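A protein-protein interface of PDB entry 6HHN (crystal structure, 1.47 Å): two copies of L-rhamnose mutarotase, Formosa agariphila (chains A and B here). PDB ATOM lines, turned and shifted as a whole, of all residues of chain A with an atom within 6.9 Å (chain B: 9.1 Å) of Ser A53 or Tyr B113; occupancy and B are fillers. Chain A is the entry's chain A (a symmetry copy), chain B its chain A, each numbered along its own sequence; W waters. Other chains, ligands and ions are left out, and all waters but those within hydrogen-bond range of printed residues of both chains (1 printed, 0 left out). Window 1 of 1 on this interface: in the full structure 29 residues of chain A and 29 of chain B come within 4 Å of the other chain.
N of Ile A54 is in hydrogen-bond range of O of Phe B112, 3.0 Å away.
N of Glu A51 is in hydrogen-bond range of OXT of Glu B115 (2.9 Å).
O of Ile A54 lies within hydrogen-bond range of N of Val B111 (2.8 Å).
The side-chain amino group (NZ) of Lys B68 is in salt-bridge range of the side-chain carboxylate (OE1) of Glu A51, at 2.7 Å.
OE1 of Glu B51 lies within salt-bridge range of NZ of Lys A68 (2.7 Å).
OE2 of Glu B110 sits at hydrogen-bond distance from OG of Ser A53 (2.7 Å).
The backbone carbonyl oxygen of Tyr A52 lies within hydrogen-bond range of the backbone NH of Met B114 (2.9 Å).
The backbone carbonyl oxygen (O) of Met B114 is in hydrogen-bond range of the backbone NH (N) of Glu A51, 3.3 Å away.
The backbone carbonyl oxygen (O) of Phe A66 sits at hydrogen-bond distance from the backbone NH (N) of Ser A53, 2.9 Å away.
The backbone carbonyl oxygen (O) of Lys A68 lies within hydrogen-bond range of the backbone NH (N) of Ser A50, 2.9 Å away.
NZ of Lys A68 lies within salt-bridge range of OE2 of Glu A51, at 2.9 Å.
N of Leu B108 is in hydrogen-bond range of O of Ala B16 (3.0 Å).
The backbone carbonyl oxygen of Phe A55 lies within hydrogen-bond range of the backbone NH of Phe A64, 2.8 Å away.
The guanidinium group of Arg B14 is in salt-bridge range of the side-chain carboxylate of Glu B110.
Among the printed residues, pairs that only touch across the chains: Phe A55 with Glu B109, Ser A53 with Phe B112, Tyr A52 with Tyr B113, Ser A50 with Glu B115, Ser A53 with Tyr B113, Leu A36 with Phe B112, Phe A55 with Ala B16, Phe A55 with Glu B110, Ile A54 with Glu B110, Phe A55 with Leu B108, Ser A53 with Arg B14, Phe A64 with Leu B108, Phe A66 with Phe B66, Phe A55 with Phe B66, His A33 with Phe B112, Tyr A52 with Phe B112, Lys A41 with Met B114 and Glu A51 with Glu B51.
Of the printed residues of chain B, Ser A53 touches Arg B14, Glu B110, Phe B112 and Tyr B113.
Of the printed residues of chain A, Tyr B113 touches Tyr A52 and Ser A53.
Ile A54 touches three residues of chain B.
Of the printed residues of chain B, Phe A55 touches Ala B16, Phe B66, Leu B108, Glu B109 and Glu B110.
Of the printed residues of chain A, Arg B14 touches Ser A53 (3.7 Å).
Printed residues of chain B within 4 Å of His A33: Phe B112 (3.8 Å).
Of the printed residues of chain B, Lys A68 touches Glu B51 (2.7 Å).
Leu B15 touches none of the printed residues of chain A.
The nearest residue of chain B that does not touch Ser A53 is Phe B66 (4.3 Å).
Printed residues of chain B that touch a printed residue of chain A: Arg B14, Ala B16, Glu B51, Phe B66, Lys B68, Leu B108, Glu B109, Glu B110, Val B111, Phe B112, Tyr B113, Met B114 and Glu B115.
Among the printed residues, 26 pairs touch across the chains.
Glu B51 touches its own counterpart, Glu A51.
Glu A51 touches Lys B68, and with the chains exchanged Lys A68 touches Glu B51.
Phe A66 touches its own counterpart, Phe B66.
Positions printed for both chains: 51, 66, 67 and 68.
Of the 26 pairs that touch across the chains among the printed residues, 4 have their exchanged pair printed and touching as well.
Water W1 bridges the backbone carbonyl oxygen of Tyr B113 (2.9 Å) and the side-chain amino group of Lys A41 (3.4 Å).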
ATOM      1  N   PHE A  17      11.935 -20.180  20.855  1.00  0.00           N
ATOM      2  CA  PHE A  17      12.403 -21.504  20.464  1.00  0.00           C
ATOM      3  C   PHE A  17      13.704 -21.393  19.696  1.00  0.00           C
ATOM      4  O   PHE A  17      14.033 -20.347  19.140  1.00  0.00           O
ATOM      5  CB  PHE A  17      11.347 -22.291  19.674  1.00  0.00           C
ATOM      6  CG  PHE A  17      10.692 -21.546  18.525  1.00  0.00           C
ATOM      7  CD1 PHE A  17       9.637 -20.679  18.754  1.00  0.00           C
ATOM      8  CD2 PHE A  17      11.132 -21.711  17.229  1.00  0.00           C
ATOM      9  CE1 PHE A  17       9.027 -20.001  17.702  1.00  0.00           C
ATOM     10  CE2 PHE A  17      10.514 -21.039  16.170  1.00  0.00           C
ATOM     11  CZ  PHE A  17       9.465 -20.189  16.421  1.00  0.00           C
ATOM     12  N   HIS A  33      14.038 -15.051   3.776  1.00  0.00           N
ATOM     13  CA  HIS A  33      13.127 -14.426   4.727  1.00  0.00           C
ATOM     14  C   HIS A  33      12.803 -12.988   4.357  1.00  0.00           C
ATOM     15  O   HIS A  33      11.695 -12.517   4.651  1.00  0.00           O
ATOM     16  CB  HIS A  33      13.673 -14.564   6.158  1.00  0.00           C
ATOM     17  CG  HIS A  33      13.496 -15.943   6.687  1.00  0.00           C
ATOM     18  ND1 HIS A  33      12.465 -16.298   7.534  1.00  0.00           N
ATOM     19  CD2 HIS A  33      14.153 -17.088   6.386  1.00  0.00           C
ATOM     20  CE1 HIS A  33      12.514 -17.601   7.757  1.00  0.00           C
ATOM     21  NE2 HIS A  33      13.528 -18.102   7.072  1.00  0.00           N
ATOM     22  N   LEU A  36       9.828 -13.476   2.295  1.00  0.00           N
ATOM     23  CA  LEU A  36       8.825 -14.358   2.879  1.00  0.00           C
ATOM     24  C   LEU A  36       7.497 -14.161   2.177  1.00  0.00           C
ATOM     25  O   LEU A  36       7.071 -13.030   1.935  1.00  0.00           O
ATOM     26  CB  LEU A  36       8.653 -14.036   4.363  1.00  0.00           C
ATOM     27  CG  LEU A  36       7.645 -14.901   5.132  1.00  0.00           C
ATOM     28  CD1 LEU A  36       8.219 -16.286   5.332  1.00  0.00           C
ATOM     29  CD2 LEU A  36       7.267 -14.287   6.453  1.00  0.00           C
ATOM     30  N   LYS A  41       2.858 -14.666   5.768  1.00  0.00           N
ATOM     31  CA  LYS A  41       2.734 -13.577   6.731  1.00  0.00           C
ATOM     32  C   LYS A  41       1.280 -13.422   7.165  1.00  0.00           C
ATOM     33  O   LYS A  41       0.978 -13.325   8.362  1.00  0.00           O
ATOM     34  CB  LYS A  41       3.260 -12.273   6.133  1.00  0.00           C
ATOM     35  CG  LYS A  41       4.765 -12.238   5.893  1.00  0.00           C
ATOM     36  CD  LYS A  41       5.198 -10.857   5.404  1.00  0.00           C
ATOM     37  CE  LYS A  41       6.554 -10.895   4.717  1.00  0.00           C
ATOM     38  NZ  LYS A  41       7.000  -9.529   4.304  1.00  0.00           N
ATOM     39  N   SER A  50       2.302 -12.145  16.357  1.00  0.00           N
ATOM     40  CA  SER A  50       2.813 -10.804  16.124  1.00  0.00           C
ATOM     41  C   SER A  50       4.229 -10.713  16.669  1.00  0.00           C
ATOM     42  O   SER A  50       4.688 -11.582  17.423  1.00  0.00           O
ATOM     43  CB  SER A  50       1.934  -9.737  16.786  1.00  0.00           C
ATOM     44  OG  SER A  50       1.921  -9.885  18.198  1.00  0.00           O
ATOM     45  N   GLU A  51       4.924  -9.654  16.256  1.00  0.00           N
ATOM     46  CA  GLU A  51       6.261  -9.334  16.750  1.00  0.00           C
ATOM     47  C   GLU A  51       7.165 -10.561  16.737  1.00  0.00           C
ATOM     48  O   GLU A  51       7.797 -10.920  17.734  1.00  0.00           O
ATOM     49  CB  GLU A  51       6.191  -8.696  18.128  1.00  0.00           C
ATOM     50  CG  GLU A  51       5.448  -7.371  18.095  1.00  0.00           C
ATOM     51  CD  GLU A  51       5.414  -6.695  19.439  1.00  0.00           C
ATOM     52  OE1 GLU A  51       6.497  -6.556  20.044  1.00  0.00           O
ATOM     53  OE2 GLU A  51       4.306  -6.328  19.890  1.00  0.00           O
ATOM     54  N   TYR A  52       7.206 -11.203  15.585  1.00  0.00           N
ATOM     55  CA  TYR A  52       7.977 -12.425  15.365  1.00  0.00           C
ATOM     56  C   TYR A  52       9.359 -12.036  14.863  1.00  0.00           C
ATOM     57  O   TYR A  52       9.498 -11.530  13.751  1.00  0.00           O
ATOM     58  CB  TYR A  52       7.241 -13.253  14.312  1.00  0.00           C
ATOM     59  CG  TYR A  52       7.780 -14.625  13.993  1.00  0.00           C
ATOM     60  CD1 TYR A  52       8.864 -15.184  14.657  1.00  0.00           C
ATOM     61  CD2 TYR A  52       7.177 -15.373  12.993  1.00  0.00           C
ATOM     62  CE1 TYR A  52       9.307 -16.451  14.330  1.00  0.00           C
ATOM     63  CE2 TYR A  52       7.611 -16.616  12.669  1.00  0.00           C
ATOM     64  CZ  TYR A  52       8.689 -17.165  13.330  1.00  0.00           C
ATOM     65  OH  TYR A  52       9.123 -18.441  12.981  1.00  0.00           O
ATOM     66  N   SER A  53      10.377 -12.282  15.690  1.00  0.00           N
ATOM     67  CA  SER A  53      11.760 -12.033  15.351  1.00  0.00           C
ATOM     68  C   SER A  53      12.532 -13.344  15.360  1.00  0.00           C
ATOM     69  O   SER A  53      12.260 -14.228  16.178  1.00  0.00           O
ATOM     70  CB  SER A  53      12.452 -11.154  16.412  1.00  0.00           C
ATOM     71  OG  SER A  53      12.051  -9.785  16.303  1.00  0.00           O
ATOM     72  N   ILE A  54      13.490 -13.459  14.447  1.00  0.00           N
ATOM     73  CA  ILE A  54      14.460 -14.550  14.484  1.00  0.00           C
ATOM     74  C   ILE A  54      15.855 -13.929  14.455  1.00  0.00           C
ATOM     75  O   ILE A  54      16.126 -13.045  13.632  1.00  0.00           O
ATOM     76  CB  ILE A  54      14.271 -15.540  13.321  1.00  0.00           C
ATOM     77  CG1 ILE A  54      12.852 -16.100  13.324  1.00  0.00           C
ATOM     78  CG2 ILE A  54      15.324 -16.671  13.442  1.00  0.00           C
ATOM     79  CD1 ILE A  54      12.494 -16.903  12.084  1.00  0.00           C
ATOM     80  N   PHE A  55      16.712 -14.353  15.400  1.00  0.00           N
ATOM     81  CA  PHE A  55      18.079 -13.883  15.552  1.00  0.00           C
ATOM     82  C   PHE A  55      19.036 -15.046  15.324  1.00  0.00           C
ATOM     83  O   PHE A  55      18.689 -16.210  15.568  1.00  0.00           O
ATOM     84  CB  PHE A  55      18.297 -13.346  16.988  1.00  0.00           C
ATOM     85  CG  PHE A  55      17.330 -12.271  17.403  1.00  0.00           C
ATOM     86  CD1 PHE A  55      16.118 -12.602  17.992  1.00  0.00           C
ATOM     87  CD2 PHE A  55      17.630 -10.940  17.211  1.00  0.00           C
ATOM     88  CE1 PHE A  55      15.230 -11.626  18.390  1.00  0.00           C
ATOM     89  CE2 PHE A  55      16.737  -9.945  17.600  1.00  0.00           C
ATOM     90  CZ  PHE A  55      15.533 -10.291  18.186  1.00  0.00           C
ATOM     91  N   PHE A  64      17.540 -18.223  17.184  1.00  0.00           N
ATOM     92  CA  PHE A  64      16.698 -17.998  18.350  1.00  0.00           C
ATOM     93  C   PHE A  64      15.498 -17.181  17.898  1.00  0.00           C
ATOM     94  O   PHE A  64      15.654 -16.054  17.414  1.00  0.00           O
ATOM     95  CB  PHE A  64      17.495 -17.276  19.432  1.00  0.00           C
ATOM     96  CG  PHE A  64      18.620 -18.104  20.023  1.00  0.00           C
ATOM     97  CD1 PHE A  64      18.382 -18.950  21.097  1.00  0.00           C
ATOM     98  CD2 PHE A  64      19.919 -18.023  19.526  1.00  0.00           C
ATOM     99  CE1 PHE A  64      19.402 -19.695  21.667  1.00  0.00           C
ATOM    100  CE2 PHE A  64      20.959 -18.772  20.101  1.00  0.00           C
ATOM    101  CZ  PHE A  64      20.692 -19.613  21.163  1.00  0.00           C
ATOM    102  N   ALA A  65      14.309 -17.749  18.050  1.00  0.00           N
ATOM    103  CA  ALA A  65      13.060 -17.128  17.634  1.00  0.00           C
ATOM    104  C   ALA A  65      12.280 -16.664  18.853  1.00  0.00           C
ATOM    105  O   ALA A  65      12.216 -17.365  19.874  1.00  0.00           O
ATOM    106  CB  ALA A  65      12.209 -18.136  16.855  1.00  0.00           C
ATOM    107  N   PHE A  66      11.669 -15.480  18.724  1.00  0.00           N
ATOM    108  CA  PHE A  66      10.772 -14.906  19.713  1.00  0.00           C
ATOM    109  C   PHE A  66       9.506 -14.471  18.988  1.00  0.00           C
ATOM    110  O   PHE A  66       9.587 -13.875  17.919  1.00  0.00           O
ATOM    111  CB  PHE A  66      11.431 -13.678  20.358  1.00  0.00           C
ATOM    112  CG  PHE A  66      10.508 -12.882  21.235  1.00  0.00           C
ATOM    113  CD1 PHE A  66       9.723 -11.858  20.707  1.00  0.00           C
ATOM    114  CD2 PHE A  66      10.400 -13.173  22.577  1.00  0.00           C
ATOM    115  CE1 PHE A  66       8.856 -11.144  21.511  1.00  0.00           C
ATOM    116  CE2 PHE A  66       9.539 -12.434  23.393  1.00  0.00           C
ATOM    117  CZ  PHE A  66       8.768 -11.427  22.850  1.00  0.00           C
ATOM    118  N   GLN A  67       8.342 -14.753  19.569  1.00  0.00           N
ATOM    119  CA  GLN A  67       7.103 -14.235  19.005  1.00  0.00           C
ATOM    120  C   GLN A  67       6.074 -14.071  20.108  1.00  0.00           C
ATOM    121  O   GLN A  67       6.187 -14.649  21.196  1.00  0.00           O
ATOM    122  CB  GLN A  67       6.552 -15.119  17.880  1.00  0.00           C
ATOM    123  CG  GLN A  67       6.228 -16.498  18.321  1.00  0.00           C
ATOM    124  CD  GLN A  67       5.819 -17.463  17.193  1.00  0.00           C
ATOM    125  OE1 GLN A  67       6.234 -17.356  16.027  1.00  0.00           O
ATOM    126  NE2 GLN A  67       5.027 -18.417  17.561  1.00  0.00           N
ATOM    127  N   LYS A  68       5.071 -13.258  19.818  1.00  0.00           N
ATOM    128  CA  LYS A  68       3.888 -13.142  20.651  1.00  0.00           C
ATOM    129  C   LYS A  68       2.738 -13.848  19.957  1.00  0.00           C
ATOM    130  O   LYS A  68       2.601 -13.769  18.733  1.00  0.00           O
ATOM    131  CB  LYS A  68       3.498 -11.689  20.859  1.00  0.00           C
ATOM    132  CG  LYS A  68       4.490 -10.896  21.656  1.00  0.00           C
ATOM    133  CD  LYS A  68       3.952  -9.503  21.868  1.00  0.00           C
ATOM    134  CE  LYS A  68       5.005  -8.611  22.461  1.00  0.00           C
ATOM    135  NZ  LYS A  68       4.504  -7.212  22.667  1.00  0.00           N
ATOM    136  N   SER B  12      12.148   0.911  20.499  1.00  0.00           N
ATOM    137  CA  SER B  12      12.194   1.205  19.072  1.00  0.00           C
ATOM    138  C   SER B  12      13.144   0.236  18.373  1.00  0.00           C
ATOM    139  O   SER B  12      12.967  -0.076  17.197  1.00  0.00           O
ATOM    140  CB  SER B  12      12.643   2.647  18.814  1.00  0.00           C
ATOM    141  OG  SER B  12      11.832   3.575  19.515  1.00  0.00           O
ATOM    142  N   GLU B  13      14.159  -0.228  19.098  1.00  0.00           N
ATOM    143  CA  GLU B  13      15.105  -1.213  18.582  1.00  0.00           C
ATOM    144  C   GLU B  13      14.911  -2.522  19.334  1.00  0.00           C
ATOM    145  O   GLU B  13      14.623  -2.519  20.531  1.00  0.00           O
ATOM    146  CB  GLU B  13      16.542  -0.727  18.747  1.00  0.00           C
ATOM    147  CG  GLU B  13      16.863   0.513  17.930  1.00  0.00           C
ATOM    148  CD  GLU B  13      16.896   0.235  16.438  1.00  0.00           C
ATOM    149  OE1 GLU B  13      16.939  -0.954  16.052  1.00  0.00           O
ATOM    150  OE2 GLU B  13      16.882   1.205  15.650  1.00  0.00           O
ATOM    151  N   ARG B  14      15.064  -3.641  18.636  1.00  0.00           N
ATOM    152  CA  ARG B  14      15.031  -4.952  19.274  1.00  0.00           C
ATOM    153  C   ARG B  14      16.455  -5.459  19.425  1.00  0.00           C
ATOM    154  O   ARG B  14      17.237  -5.396  18.465  1.00  0.00           O
ATOM    155  CB  ARG B  14      14.209  -5.933  18.439  1.00  0.00           C
ATOM    156  CG  ARG B  14      12.769  -5.458  18.252  1.00  0.00           C
ATOM    157  CD  ARG B  14      12.039  -6.234  17.183  1.00  0.00           C
ATOM    158  NE  ARG B  14      12.642  -6.091  15.866  1.00  0.00           N
ATOM    159  CZ  ARG B  14      12.406  -5.084  15.026  1.00  0.00           C
ATOM    160  NH1 ARG B  14      13.004  -5.064  13.842  1.00  0.00           N
ATOM    161  NH2 ARG B  14      11.587  -4.102  15.362  1.00  0.00           N
ATOM    162  N   LEU B  15      16.771  -5.984  20.598  1.00  0.00           N
ATOM    163  CA  LEU B  15      18.085  -6.520  20.890  1.00  0.00           C
ATOM    164  C   LEU B  15      17.943  -7.928  21.443  1.00  0.00           C
ATOM    165  O   LEU B  15      17.033  -8.208  22.225  1.00  0.00           O
ATOM    166  CB  LEU B  15      18.796  -5.680  21.959  1.00  0.00           C
ATOM    167  CG  LEU B  15      19.303  -4.301  21.583  1.00  0.00           C
ATOM    168  CD1 LEU B  15      20.128  -3.809  22.767  1.00  0.00           C
ATOM    169  CD2 LEU B  15      20.098  -4.321  20.302  1.00  0.00           C
ATOM    170  N   ALA B  16      18.854  -8.806  21.058  1.00  0.00           N
ATOM    171  CA  ALA B  16      18.898 -10.138  21.632  1.00  0.00           C
ATOM    172  C   ALA B  16      20.341 -10.518  21.909  1.00  0.00           C
ATOM    173  O   ALA B  16      21.260 -10.126  21.176  1.00  0.00           O
ATOM    174  CB  ALA B  16      18.275 -11.175  20.683  1.00  0.00           C
ATOM    175  N   GLU B  51       9.810  -4.714  27.709  1.00  0.00           N
ATOM    176  CA  GLU B  51       9.529  -6.056  27.206  1.00  0.00           C
ATOM    177  C   GLU B  51      10.785  -6.920  27.199  1.00  0.00           C
ATOM    178  O   GLU B  51      11.154  -7.530  26.193  1.00  0.00           O
ATOM    179  CB  GLU B  51       8.876  -5.994  25.834  1.00  0.00           C
ATOM    180  CG  GLU B  51       7.527  -5.295  25.886  1.00  0.00           C
ATOM    181  CD  GLU B  51       6.838  -5.271  24.548  1.00  0.00           C
ATOM    182  OE1 GLU B  51       6.729  -6.352  23.935  1.00  0.00           O
ATOM    183  OE2 GLU B  51       6.432  -4.171  24.111  1.00  0.00           O
ATOM    184  N   PHE B  66      15.829 -11.242  25.125  1.00  0.00           N
ATOM    185  CA  PHE B  66      15.217 -10.356  24.150  1.00  0.00           C
ATOM    186  C   PHE B  66      14.747  -9.111  24.891  1.00  0.00           C
ATOM    187  O   PHE B  66      14.164  -9.221  25.965  1.00  0.00           O
ATOM    188  CB  PHE B  66      14.004 -11.049  23.510  1.00  0.00           C
ATOM    189  CG  PHE B  66      13.171 -10.144  22.649  1.00  0.00           C
ATOM    190  CD1 PHE B  66      12.127  -9.398  23.194  1.00  0.00           C
ATOM    191  CD2 PHE B  66      13.446 -10.015  21.306  1.00  0.00           C
ATOM    192  CE1 PHE B  66      11.377  -8.547  22.404  1.00  0.00           C
ATOM    193  CE2 PHE B  66      12.671  -9.171  20.505  1.00  0.00           C
ATOM    194  CZ  PHE B  66      11.645  -8.438  21.063  1.00  0.00           C
ATOM    195  N   GLN B  67      14.986  -7.934  24.318  1.00  0.00           N
ATOM    196  CA  GLN B  67      14.433  -6.717  24.898  1.00  0.00           C
ATOM    197  C   GLN B  67      14.226  -5.684  23.806  1.00  0.00           C
ATOM    198  O   GLN B  67      14.796  -5.768  22.712  1.00  0.00           O
ATOM    199  CB  GLN B  67      15.309  -6.148  26.021  1.00  0.00           C
ATOM    200  CG  GLN B  67      16.673  -5.776  25.571  1.00  0.00           C
ATOM    201  CD  GLN B  67      17.634  -5.345  26.693  1.00  0.00           C
ATOM    202  OE1 GLN B  67      17.552  -5.774  27.857  1.00  0.00           O
ATOM    203  NE2 GLN B  67      18.559  -4.519  26.324  1.00  0.00           N
ATOM    204  N   LYS B  68      13.383  -4.711  24.113  1.00  0.00           N
ATOM    205  CA  LYS B  68      13.221  -3.525  23.292  1.00  0.00           C
ATOM    206  C   LYS B  68      13.895  -2.358  23.991  1.00  0.00           C
ATOM    207  O   LYS B  68      13.824  -2.235  25.216  1.00  0.00           O
ATOM    208  CB  LYS B  68      11.755  -3.180  23.102  1.00  0.00           C
ATOM    209  CG  LYS B  68      10.986  -4.190  22.302  1.00  0.00           C
ATOM    210  CD  LYS B  68       9.575  -3.697  22.108  1.00  0.00           C
ATOM    211  CE  LYS B  68       8.712  -4.773  21.513  1.00  0.00           C
ATOM    212  NZ  LYS B  68       7.296  -4.315  21.324  1.00  0.00           N
ATOM    213  N   LEU B 108      23.239 -11.404  19.309  1.00  0.00           N
ATOM    214  CA  LEU B 108      22.578 -12.168  18.261  1.00  0.00           C
ATOM    215  C   LEU B 108      21.953 -11.208  17.261  1.00  0.00           C
ATOM    216  O   LEU B 108      21.203 -10.307  17.645  1.00  0.00           O
ATOM    217  CB  LEU B 108      21.508 -13.059  18.873  1.00  0.00           C
ATOM    218  CG  LEU B 108      21.995 -13.995  19.983  1.00  0.00           C
ATOM    219  CD1 LEU B 108      20.829 -14.661  20.711  1.00  0.00           C
ATOM    220  CD2 LEU B 108      22.915 -15.028  19.424  1.00  0.00           C
ATOM    221  N   GLU B 109      22.238 -11.425  15.980  1.00  0.00           N
ATOM    222  CA  GLU B 109      21.828 -10.517  14.914  1.00  0.00           C
ATOM    223  C   GLU B 109      20.434 -10.878  14.408  1.00  0.00           C
ATOM    224  O   GLU B 109      20.161 -12.041  14.097  1.00  0.00           O
ATOM    225  CB  GLU B 109      22.837 -10.644  13.768  1.00  0.00           C
ATOM    226  CG  GLU B 109      22.535  -9.818  12.524  1.00  0.00           C
ATOM    227  CD  GLU B 109      23.482 -10.137  11.365  1.00  0.00           C
ATOM    228  OE1 GLU B 109      24.595 -10.654  11.617  1.00  0.00           O
ATOM    229  OE2 GLU B 109      23.117  -9.879  10.198  1.00  0.00           O
ATOM    230  N   GLU B 110      19.555  -9.877  14.306  1.00  0.00           N
ATOM    231  CA  GLU B 110      18.218 -10.143  13.778  1.00  0.00           C
ATOM    232  C   GLU B 110      18.285 -10.428  12.281  1.00  0.00           C
ATOM    233  O   GLU B 110      18.868  -9.653  11.516  1.00  0.00           O
ATOM    234  CB  GLU B 110      17.275  -8.973  14.053  1.00  0.00           C
ATOM    235  CG  GLU B 110      15.820  -9.347  13.843  1.00  0.00           C
ATOM    236  CD  GLU B 110      14.871  -8.216  14.168  1.00  0.00           C
ATOM    237  OE1 GLU B 110      14.977  -7.151  13.517  1.00  0.00           O
ATOM    238  OE2 GLU B 110      14.016  -8.403  15.067  1.00  0.00           O
ATOM    239  N   VAL B 111      17.699 -11.552  11.870  1.00  0.00           N
ATOM    240  CA  VAL B 111      17.653 -11.944  10.464  1.00  0.00           C
ATOM    241  C   VAL B 111      16.237 -12.002   9.900  1.00  0.00           C
ATOM    242  O   VAL B 111      16.078 -12.202   8.682  1.00  0.00           O
ATOM    243  CB  VAL B 111      18.392 -13.270  10.202  1.00  0.00           C
ATOM    244  CG1 VAL B 111      19.901 -13.087  10.401  1.00  0.00           C
ATOM    245  CG2 VAL B 111      17.889 -14.378  11.099  1.00  0.00           C
ATOM    246  N   PHE B 112      15.215 -11.852  10.739  1.00  0.00           N
ATOM    247  CA  PHE B 112      13.832 -11.792  10.282  1.00  0.00           C
ATOM    248  C   PHE B 112      13.023 -11.024  11.312  1.00  0.00           C
ATOM    249  O   PHE B 112      13.213 -11.214  12.514  1.00  0.00           O
ATOM    250  CB  PHE B 112      13.253 -13.198  10.117  1.00  0.00           C
ATOM    251  CG  PHE B 112      11.786 -13.219   9.813  1.00  0.00           C
ATOM    252  CD1 PHE B 112      11.308 -12.787   8.581  1.00  0.00           C
ATOM    253  CD2 PHE B 112      10.878 -13.672  10.750  1.00  0.00           C
ATOM    254  CE1 PHE B 112       9.955 -12.819   8.307  1.00  0.00           C
ATOM    255  CE2 PHE B 112       9.516 -13.685  10.475  1.00  0.00           C
ATOM    256  CZ  PHE B 112       9.066 -13.269   9.253  1.00  0.00           C
ATOM    257  N   TYR B 113      12.103 -10.175  10.826  1.00  0.00           N
ATOM    258  CA  TYR B 113      11.116  -9.544  11.684  1.00  0.00           C
ATOM    259  C   TYR B 113       9.803  -9.398  10.931  1.00  0.00           C
ATOM    260  O   TYR B 113       9.788  -8.898   9.802  1.00  0.00           O
ATOM    261  CB  TYR B 113      11.588  -8.169  12.174  1.00  0.00           C
ATOM    262  CG  TYR B 113      10.543  -7.410  12.975  1.00  0.00           C
ATOM    263  CD1 TYR B 113      10.144  -7.840  14.238  1.00  0.00           C
ATOM    264  CD2 TYR B 113       9.962  -6.264  12.469  1.00  0.00           C
ATOM    265  CE1 TYR B 113       9.201  -7.155  14.971  1.00  0.00           C
ATOM    266  CE2 TYR B 113       9.016  -5.569  13.192  1.00  0.00           C
ATOM    267  CZ  TYR B 113       8.641  -6.022  14.441  1.00  0.00           C
ATOM    268  OH  TYR B 113       7.694  -5.332  15.156  1.00  0.00           O
ATOM    269  N   MET B 114       8.714  -9.822  11.576  1.00  0.00           N
ATOM    270  CA  MET B 114       7.349  -9.556  11.113  1.00  0.00           C
ATOM    271  C   MET B 114       6.572  -8.929  12.264  1.00  0.00           C
ATOM    272  O   MET B 114       6.369  -9.572  13.299  1.00  0.00           O
ATOM    273  CB  MET B 114       6.663 -10.853  10.657  1.00  0.00           C
ATOM    274  CG  MET B 114       5.283 -10.624  10.082  1.00  0.00           C
ATOM    275  SD  MET B 114       4.209 -12.074  10.123  1.00  0.00           S
ATOM    276  CE  MET B 114       3.897 -12.217  11.879  1.00  0.00           C
ATOM    277  N   GLU B 115       6.113  -7.699  12.079  1.00  0.00           N
ATOM    278  CA  GLU B 115       5.315  -7.041  13.114  1.00  0.00           C
ATOM    279  C   GLU B 115       3.966  -7.745  13.305  1.00  0.00           C
ATOM    280  O   GLU B 115       3.322  -8.145  12.327  1.00  0.00           O
ATOM    281  CB  GLU B 115       5.077  -5.578  12.763  1.00  0.00           C
ATOM    282  CG  GLU B 115       4.241  -4.840  13.799  1.00  0.00           C
ATOM    283  CD  GLU B 115       3.841  -3.446  13.343  1.00  0.00           C
ATOM    284  OE1 GLU B 115       4.719  -2.708  12.849  1.00  0.00           O
ATOM    285  OE2 GLU B 115       2.646  -3.099  13.467  1.00  0.00           O
ATOM    286  OXT GLU B 115       3.498  -7.904  14.443  1.00  0.00           O
HETATM  287  O   HOH W   1       8.239  -9.638   7.470  1.00  0.00           O
